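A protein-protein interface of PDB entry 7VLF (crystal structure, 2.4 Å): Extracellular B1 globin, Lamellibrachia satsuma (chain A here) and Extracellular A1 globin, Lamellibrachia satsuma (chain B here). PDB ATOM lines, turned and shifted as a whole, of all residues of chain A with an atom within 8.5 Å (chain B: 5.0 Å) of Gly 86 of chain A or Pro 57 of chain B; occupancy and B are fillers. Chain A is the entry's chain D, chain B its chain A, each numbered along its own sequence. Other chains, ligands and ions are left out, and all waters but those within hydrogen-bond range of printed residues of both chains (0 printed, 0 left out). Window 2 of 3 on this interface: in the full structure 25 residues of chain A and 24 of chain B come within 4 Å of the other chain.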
ATOM      1  N   SER A   1      16.215  28.817  10.704  1.00  0.00           N
ATOM      2  CA  SER A   1      16.059  29.692   9.548  1.00  0.00           C
ATOM      3  C   SER A   1      15.829  28.878   8.279  1.00  0.00           C
ATOM      4  O   SER A   1      14.832  29.063   7.585  1.00  0.00           O
ATOM      5  CB  SER A   1      17.283  30.594   9.382  1.00  0.00           C
ATOM      6  OG  SER A   1      17.106  31.505   8.310  1.00  0.00           O
ATOM      7  N   GLU A   2      16.759  27.977   7.979  1.00  0.00           N
ATOM      8  CA  GLU A   2      16.650  27.081   6.838  1.00  0.00           C
ATOM      9  C   GLU A   2      16.477  25.648   7.322  1.00  0.00           C
ATOM     10  O   GLU A   2      17.146  25.217   8.266  1.00  0.00           O
ATOM     11  CB  GLU A   2      17.879  27.185   5.938  1.00  0.00           C
ATOM     12  CG  GLU A   2      17.577  27.635   4.518  1.00  0.00           C
ATOM     13  CD  GLU A   2      16.930  26.551   3.668  1.00  0.00           C
ATOM     14  OE1 GLU A   2      16.578  26.849   2.510  1.00  0.00           O
ATOM     15  OE2 GLU A   2      16.776  25.406   4.146  1.00  0.00           O
ATOM     16  N   PHE A   3      15.588  24.906   6.661  1.00  0.00           N
ATOM     17  CA  PHE A   3      15.231  23.562   7.100  1.00  0.00           C
ATOM     18  C   PHE A   3      15.896  22.481   6.249  1.00  0.00           C
ATOM     19  O   PHE A   3      16.678  21.677   6.766  1.00  0.00           O
ATOM     20  CB  PHE A   3      13.706  23.411   7.094  1.00  0.00           C
ATOM     21  CG  PHE A   3      13.015  24.236   8.144  1.00  0.00           C
ATOM     22  CD1 PHE A   3      12.814  25.596   7.955  1.00  0.00           C
ATOM     23  CD2 PHE A   3      12.566  23.655   9.320  1.00  0.00           C
ATOM     24  CE1 PHE A   3      12.179  26.358   8.915  1.00  0.00           C
ATOM     25  CE2 PHE A   3      11.928  24.412  10.286  1.00  0.00           C
ATOM     26  CZ  PHE A   3      11.734  25.767  10.082  1.00  0.00           C
ATOM     27  N   TYR A  81       4.916  22.770   3.538  1.00  0.00           N
ATOM     28  CA  TYR A  81       5.484  24.103   3.689  1.00  0.00           C
ATOM     29  C   TYR A  81       6.996  24.075   3.866  1.00  0.00           C
ATOM     30  O   TYR A  81       7.580  25.070   4.307  1.00  0.00           O
ATOM     31  CB  TYR A  81       4.833  24.827   4.867  1.00  0.00           C
ATOM     32  CG  TYR A  81       3.538  25.525   4.525  1.00  0.00           C
ATOM     33  CD1 TYR A  81       2.348  24.818   4.436  1.00  0.00           C
ATOM     34  CD2 TYR A  81       3.504  26.897   4.304  1.00  0.00           C
ATOM     35  CE1 TYR A  81       1.160  25.454   4.131  1.00  0.00           C
ATOM     36  CE2 TYR A  81       2.321  27.543   3.998  1.00  0.00           C
ATOM     37  CZ  TYR A  81       1.153  26.817   3.913  1.00  0.00           C
ATOM     38  OH  TYR A  81      -0.028  27.456   3.609  1.00  0.00           O
ATOM     39  N   LEU A  82       7.646  22.958   3.529  1.00  0.00           N
ATOM     40  CA  LEU A  82       9.093  22.856   3.674  1.00  0.00           C
ATOM     41  C   LEU A  82       9.837  23.846   2.788  1.00  0.00           C
ATOM     42  O   LEU A  82      10.982  24.194   3.093  1.00  0.00           O
ATOM     43  CB  LEU A  82       9.555  21.434   3.358  1.00  0.00           C
ATOM     44  CG  LEU A  82       9.357  20.368   4.436  1.00  0.00           C
ATOM     45  CD1 LEU A  82       9.598  18.983   3.858  1.00  0.00           C
ATOM     46  CD2 LEU A  82      10.282  20.624   5.613  1.00  0.00           C
ATOM     47  N   ASN A  83       9.216  24.307   1.701  1.00  0.00           N
ATOM     48  CA  ASN A  83       9.886  25.219   0.784  1.00  0.00           C
ATOM     49  C   ASN A  83       9.805  26.673   1.229  1.00  0.00           C
ATOM     50  O   ASN A  83      10.623  27.486   0.787  1.00  0.00           O
ATOM     51  CB  ASN A  83       9.296  25.069  -0.619  1.00  0.00           C
ATOM     52  CG  ASN A  83       9.541  23.694  -1.210  1.00  0.00           C
ATOM     53  OD1 ASN A  83      10.649  23.163  -1.136  1.00  0.00           O
ATOM     54  ND2 ASN A  83       8.503  23.106  -1.792  1.00  0.00           N
ATOM     55  N   ASP A  84       8.847  27.020   2.084  1.00  0.00           N
ATOM     56  CA  ASP A  84       8.727  28.373   2.623  1.00  0.00           C
ATOM     57  C   ASP A  84       9.320  28.362   4.027  1.00  0.00           C
ATOM     58  O   ASP A  84       8.690  27.892   4.977  1.00  0.00           O
ATOM     59  CB  ASP A  84       7.274  28.835   2.632  1.00  0.00           C
ATOM     60  CG  ASP A  84       7.126  30.290   3.040  1.00  0.00           C
ATOM     61  OD1 ASP A  84       8.155  30.959   3.270  1.00  0.00           O
ATOM     62  OD2 ASP A  84       5.976  30.768   3.127  1.00  0.00           O
ATOM     63  N   ALA A  85      10.540  28.885   4.155  1.00  0.00           N
ATOM     64  CA  ALA A  85      11.205  28.884   5.452  1.00  0.00           C
ATOM     65  C   ALA A  85      10.576  29.885   6.411  1.00  0.00           C
ATOM     66  O   ALA A  85      10.556  29.650   7.623  1.00  0.00           O
ATOM     67  CB  ALA A  85      12.694  29.178   5.276  1.00  0.00           C
ATOM     68  N   GLY A  86      10.059  30.999   5.891  1.00  0.00           N
ATOM     69  CA  GLY A  86       9.488  32.011   6.765  1.00  0.00           C
ATOM     70  C   GLY A  86       8.221  31.534   7.449  1.00  0.00           C
ATOM     71  O   GLY A  86       8.072  31.662   8.667  1.00  0.00           O
ATOM     72  N   THR A  87       7.290  30.976   6.673  1.00  0.00           N
ATOM     73  CA  THR A  87       6.055  30.468   7.257  1.00  0.00           C
ATOM     74  C   THR A  87       6.324  29.272   8.157  1.00  0.00           C
ATOM     75  O   THR A  87       5.723  29.143   9.230  1.00  0.00           O
ATOM     76  CB  THR A  87       5.070  30.087   6.154  1.00  0.00           C
ATOM     77  OG1 THR A  87       4.906  31.190   5.257  1.00  0.00           O
ATOM     78  CG2 THR A  87       3.723  29.724   6.751  1.00  0.00           C
ATOM     79  N   LEU A  88       7.229  28.385   7.737  1.00  0.00           N
ATOM     80  CA  LEU A  88       7.488  27.170   8.502  1.00  0.00           C
ATOM     81  C   LEU A  88       8.063  27.494   9.875  1.00  0.00           C
ATOM     82  O   LEU A  88       7.747  26.819  10.862  1.00  0.00           O
ATOM     83  CB  LEU A  88       8.429  26.257   7.721  1.00  0.00           C
ATOM     84  CG  LEU A  88       8.690  24.862   8.284  1.00  0.00           C
ATOM     85  CD1 LEU A  88       7.383  24.120   8.514  1.00  0.00           C
ATOM     86  CD2 LEU A  88       9.586  24.090   7.334  1.00  0.00           C
ATOM     87  N   THR A  89       8.909  28.523   9.960  1.00  0.00           N
ATOM     88  CA  THR A  89       9.445  28.930  11.255  1.00  0.00           C
ATOM     89  C   THR A  89       8.336  29.418  12.177  1.00  0.00           C
ATOM     90  O   THR A  89       8.305  29.070  13.363  1.00  0.00           O
ATOM     91  CB  THR A  89      10.507  30.012  11.068  1.00  0.00           C
ATOM     92  OG1 THR A  89      11.610  29.477  10.325  1.00  0.00           O
ATOM     93  CG2 THR A  89      11.004  30.506  12.418  1.00  0.00           C
ATOM     94  N   SER A  90       7.409  30.220  11.646  1.00  0.00           N
ATOM     95  CA  SER A  90       6.258  30.650  12.433  1.00  0.00           C
ATOM     96  C   SER A  90       5.357  29.472  12.782  1.00  0.00           C
ATOM     97  O   SER A  90       4.802  29.412  13.885  1.00  0.00           O
ATOM     98  CB  SER A  90       5.472  31.714  11.671  1.00  0.00           C
ATOM     99  OG  SER A  90       4.240  31.989  12.312  1.00  0.00           O
ATOM    100  N   LEU A  91       5.204  28.524  11.856  1.00  0.00           N
ATOM    101  CA  LEU A  91       4.369  27.358  12.123  1.00  0.00           C
ATOM    102  C   LEU A  91       4.986  26.465  13.191  1.00  0.00           C
ATOM    103  O   LEU A  91       4.285  25.992  14.093  1.00  0.00           O
ATOM    104  CB  LEU A  91       4.143  26.572  10.833  1.00  0.00           C
ATOM    105  CG  LEU A  91       3.108  27.143   9.863  1.00  0.00           C
ATOM    106  CD1 LEU A  91       3.139  26.395   8.539  1.00  0.00           C
ATOM    107  CD2 LEU A  91       1.721  27.078  10.479  1.00  0.00           C
ATOM    108  N   THR A  92       6.294  26.216  13.104  1.00  0.00           N
ATOM    109  CA  THR A  92       6.951  25.378  14.100  1.00  0.00           C
ATOM    110  C   THR A  92       6.970  26.040  15.471  1.00  0.00           C
ATOM    111  O   THR A  92       6.884  25.349  16.492  1.00  0.00           O
ATOM    112  CB  THR A  92       8.374  25.047  13.656  1.00  0.00           C
ATOM    113  OG1 THR A  92       9.054  26.254  13.288  1.00  0.00           O
ATOM    114  CG2 THR A  92       8.352  24.094  12.472  1.00  0.00           C
ATOM    115  N   ALA A  93       7.083  27.368  15.516  1.00  0.00           N
ATOM    116  CA  ALA A  93       7.075  28.060  16.799  1.00  0.00           C
ATOM    117  C   ALA A  93       5.714  27.973  17.475  1.00  0.00           C
ATOM    118  O   ALA A  93       5.636  27.956  18.709  1.00  0.00           O
ATOM    119  CB  ALA A  93       7.485  29.520  16.613  1.00  0.00           C
ATOM    120  N   ARG B  55       0.921  39.157   3.664  1.00  0.00           N
ATOM    121  CA  ARG B  55       2.143  38.452   3.305  1.00  0.00           C
ATOM    122  C   ARG B  55       2.991  38.083   4.512  1.00  0.00           C
ATOM    123  O   ARG B  55       4.010  37.403   4.344  1.00  0.00           O
ATOM    124  CB  ARG B  55       2.979  39.300   2.347  1.00  0.00           C
ATOM    125  CG  ARG B  55       2.200  39.891   1.187  1.00  0.00           C
ATOM    126  CD  ARG B  55       2.899  41.137   0.669  1.00  0.00           C
ATOM    127  NE  ARG B  55       3.070  42.125   1.731  1.00  0.00           N
ATOM    128  CZ  ARG B  55       3.869  43.185   1.650  1.00  0.00           C
ATOM    129  NH1 ARG B  55       4.585  43.400   0.555  1.00  0.00           N
ATOM    130  NH2 ARG B  55       3.957  44.027   2.671  1.00  0.00           N
ATOM    131  N   SER B  56       2.615  38.520   5.708  1.00  0.00           N
ATOM    132  CA  SER B  56       3.432  38.248   6.879  1.00  0.00           C
ATOM    133  C   SER B  56       3.402  36.756   7.196  1.00  0.00           C
ATOM    134  O   SER B  56       2.368  36.105   7.012  1.00  0.00           O
ATOM    135  CB  SER B  56       2.933  39.044   8.081  1.00  0.00           C
ATOM    136  OG  SER B  56       1.796  38.420   8.653  1.00  0.00           O
ATOM    137  N   PRO B  57       4.515  36.185   7.661  1.00  0.00           N
ATOM    138  CA  PRO B  57       4.510  34.752   7.997  1.00  0.00           C
ATOM    139  C   PRO B  57       3.602  34.415   9.160  1.00  0.00           C
ATOM    140  O   PRO B  57       3.280  33.238   9.355  1.00  0.00           O
ATOM    141  CB  PRO B  57       5.982  34.459   8.322  1.00  0.00           C
ATOM    142  CG  PRO B  57       6.550  35.778   8.719  1.00  0.00           C
ATOM    143  CD  PRO B  57       5.831  36.804   7.886  1.00  0.00           C
ATOM    144  N   GLN B  58       3.177  35.410   9.942  1.00  0.00           N
ATOM    145  CA  GLN B  58       2.214  35.153  11.006  1.00  0.00           C
ATOM    146  C   GLN B  58       0.823  34.903  10.437  1.00  0.00           C
ATOM    147  O   GLN B  58       0.087  34.040  10.932  1.00  0.00           O
ATOM    148  CB  GLN B  58       2.197  36.323  11.992  1.00  0.00           C
ATOM    149  CG  GLN B  58       3.477  36.468  12.807  1.00  0.00           C
ATOM    150  CD  GLN B  58       4.633  37.030  12.001  1.00  0.00           C
ATOM    151  OE1 GLN B  58       4.432  37.705  10.993  1.00  0.00           O
ATOM    152  NE2 GLN B  58       5.854  36.748  12.443  1.00  0.00           N
ATOM    153  N   PHE B  59       0.445  35.641   9.391  1.00  0.00           N
ATOM    154  CA  PHE B  59      -0.832  35.392   8.736  1.00  0.00           C
ATOM    155  C   PHE B  59      -0.752  34.221   7.765  1.00  0.00           C
ATOM    156  O   PHE B  59      -1.739  33.498   7.593  1.00  0.00           O
ATOM    157  CB  PHE B  59      -1.308  36.649   8.009  1.00  0.00           C
ATOM    158  CG  PHE B  59      -2.676  36.516   7.407  1.00  0.00           C
ATOM    159  CD1 PHE B  59      -3.785  36.319   8.212  1.00  0.00           C
ATOM    160  CD2 PHE B  59      -2.854  36.592   6.037  1.00  0.00           C
ATOM    161  CE1 PHE B  59      -5.047  36.195   7.663  1.00  0.00           C
ATOM    162  CE2 PHE B  59      -4.113  36.474   5.479  1.00  0.00           C
ATOM    163  CZ  PHE B  59      -5.212  36.273   6.293  1.00  0.00           C
ATOM    164  N   LYS B  60       0.404  34.017   7.125  1.00  0.00           N
ATOM    165  CA  LYS B  60       0.585  32.823   6.309  1.00  0.00           C
ATOM    166  C   LYS B  60       0.494  31.560   7.152  1.00  0.00           C
ATOM    167  O   LYS B  60       0.030  30.521   6.668  1.00  0.00           O
ATOM    168  CB  LYS B  60       1.926  32.879   5.574  1.00  0.00           C
ATOM    169  CG  LYS B  60       1.989  33.925   4.470  1.00  0.00           C
ATOM    170  CD  LYS B  60       3.269  33.802   3.652  1.00  0.00           C
ATOM    171  CE  LYS B  60       4.491  34.204   4.464  1.00  0.00           C
ATOM    172  NZ  LYS B  60       5.769  33.957   3.739  1.00  0.00           N
ATOM    173  N   ALA B  61       0.927  31.629   8.413  1.00  0.00           N
ATOM    174  CA  ALA B  61       0.764  30.494   9.314  1.00  0.00           C
ATOM    175  C   ALA B  61      -0.697  30.312   9.711  1.00  0.00           C
ATOM    176  O   ALA B  61      -1.176  29.179   9.837  1.00  0.00           O
ATOM    177  CB  ALA B  61       1.641  30.678  10.551  1.00  0.00           C
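The side-chain hydroxyl (OG) of Ser 90 of chain A sits at hydrogen-bond distance from the backbone carbonyl oxygen (O) of Pro 57 of chain B, 3.4 Å away.
The side-chain amino group (NZ) of Lys 60 of chain B is in salt-bridge range of the side-chain carboxylate (OD2) of Asp 84 of chain A, at 3.3 Å.
The side-chain hydroxyl of Thr 87 of chain A sits close to the side-chain amino group of Lys 60 of chain B (3.3 Å).
OD1 of Asp 84 of chain A is in hydrogen-bond range of N of Gly 86 of chain A.
OD2 of Asp 84 of chain A sits at hydrogen-bond distance from OG1 of Thr 87 of chain A (2.4 Å).
Gly 86 of chain A touches Pro 57 of chain B (O to CB, 3.5 Å).
Ala 61 of chain B touches Thr 87 of chain A.
OG of Ser 90 of chain A touches CA of Gln 58 of chain B, 3.98 Å away.
Ser 90 of chain A touches Ala 61 of chain B (OG to CB, 3.4 Å).
CB of Ala 61 of chain B touches CD2 of Leu 91 of chain A, 3.6 Å away.
Asn 83 of chain A touches none of the printed residues of chain B.
Of chain B, only Pro 57 comes within 4 Å of Gly 86 of chain A.
Printed residues of chain B within 4 Å of Thr 87 of chain A: Lys 60 and Ala 61.
Printed residues of chain B within 4 Å of Ser 90 of chain A: Pro 57 (3.4 Å), Gln 58 (3.98 Å) and Ala 61 (3.4 Å).
Of the printed residues of chain B, Leu 91 of chain A touches Ala 61.
Ala 93 of chain A touches none of the printed residues of chain B.
Gln 58 of chain B touches just one residue of chain A: Ser 90 (3.98 Å).
Of the printed residues of chain A, Ala 61 of chain B touches Thr 87, Ser 90 and Leu 91.
Of the 16 printed residues of chain A, 5 touch a printed residue of chain B.
Hydrophobic or aromatic side chains of chain A that line the printed part of chain B: Leu 91.
Along chain A the printed residues that touch a printed residue of chain B span positions 84 to 91.
Of the 7 printed residues of chain B, 4 touch a printed residue of chain A.
Hydrophobic or aromatic side chains of chain B within 4 Å of the printed part of chain A: Pro 57 and Ala 61.
Among the printed residues, Asp or Glu carboxylates within 4 Å of a Lys or Arg side-chain nitrogen of the other chain: Asp 84 of chain A with Lys 60 of chain B.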
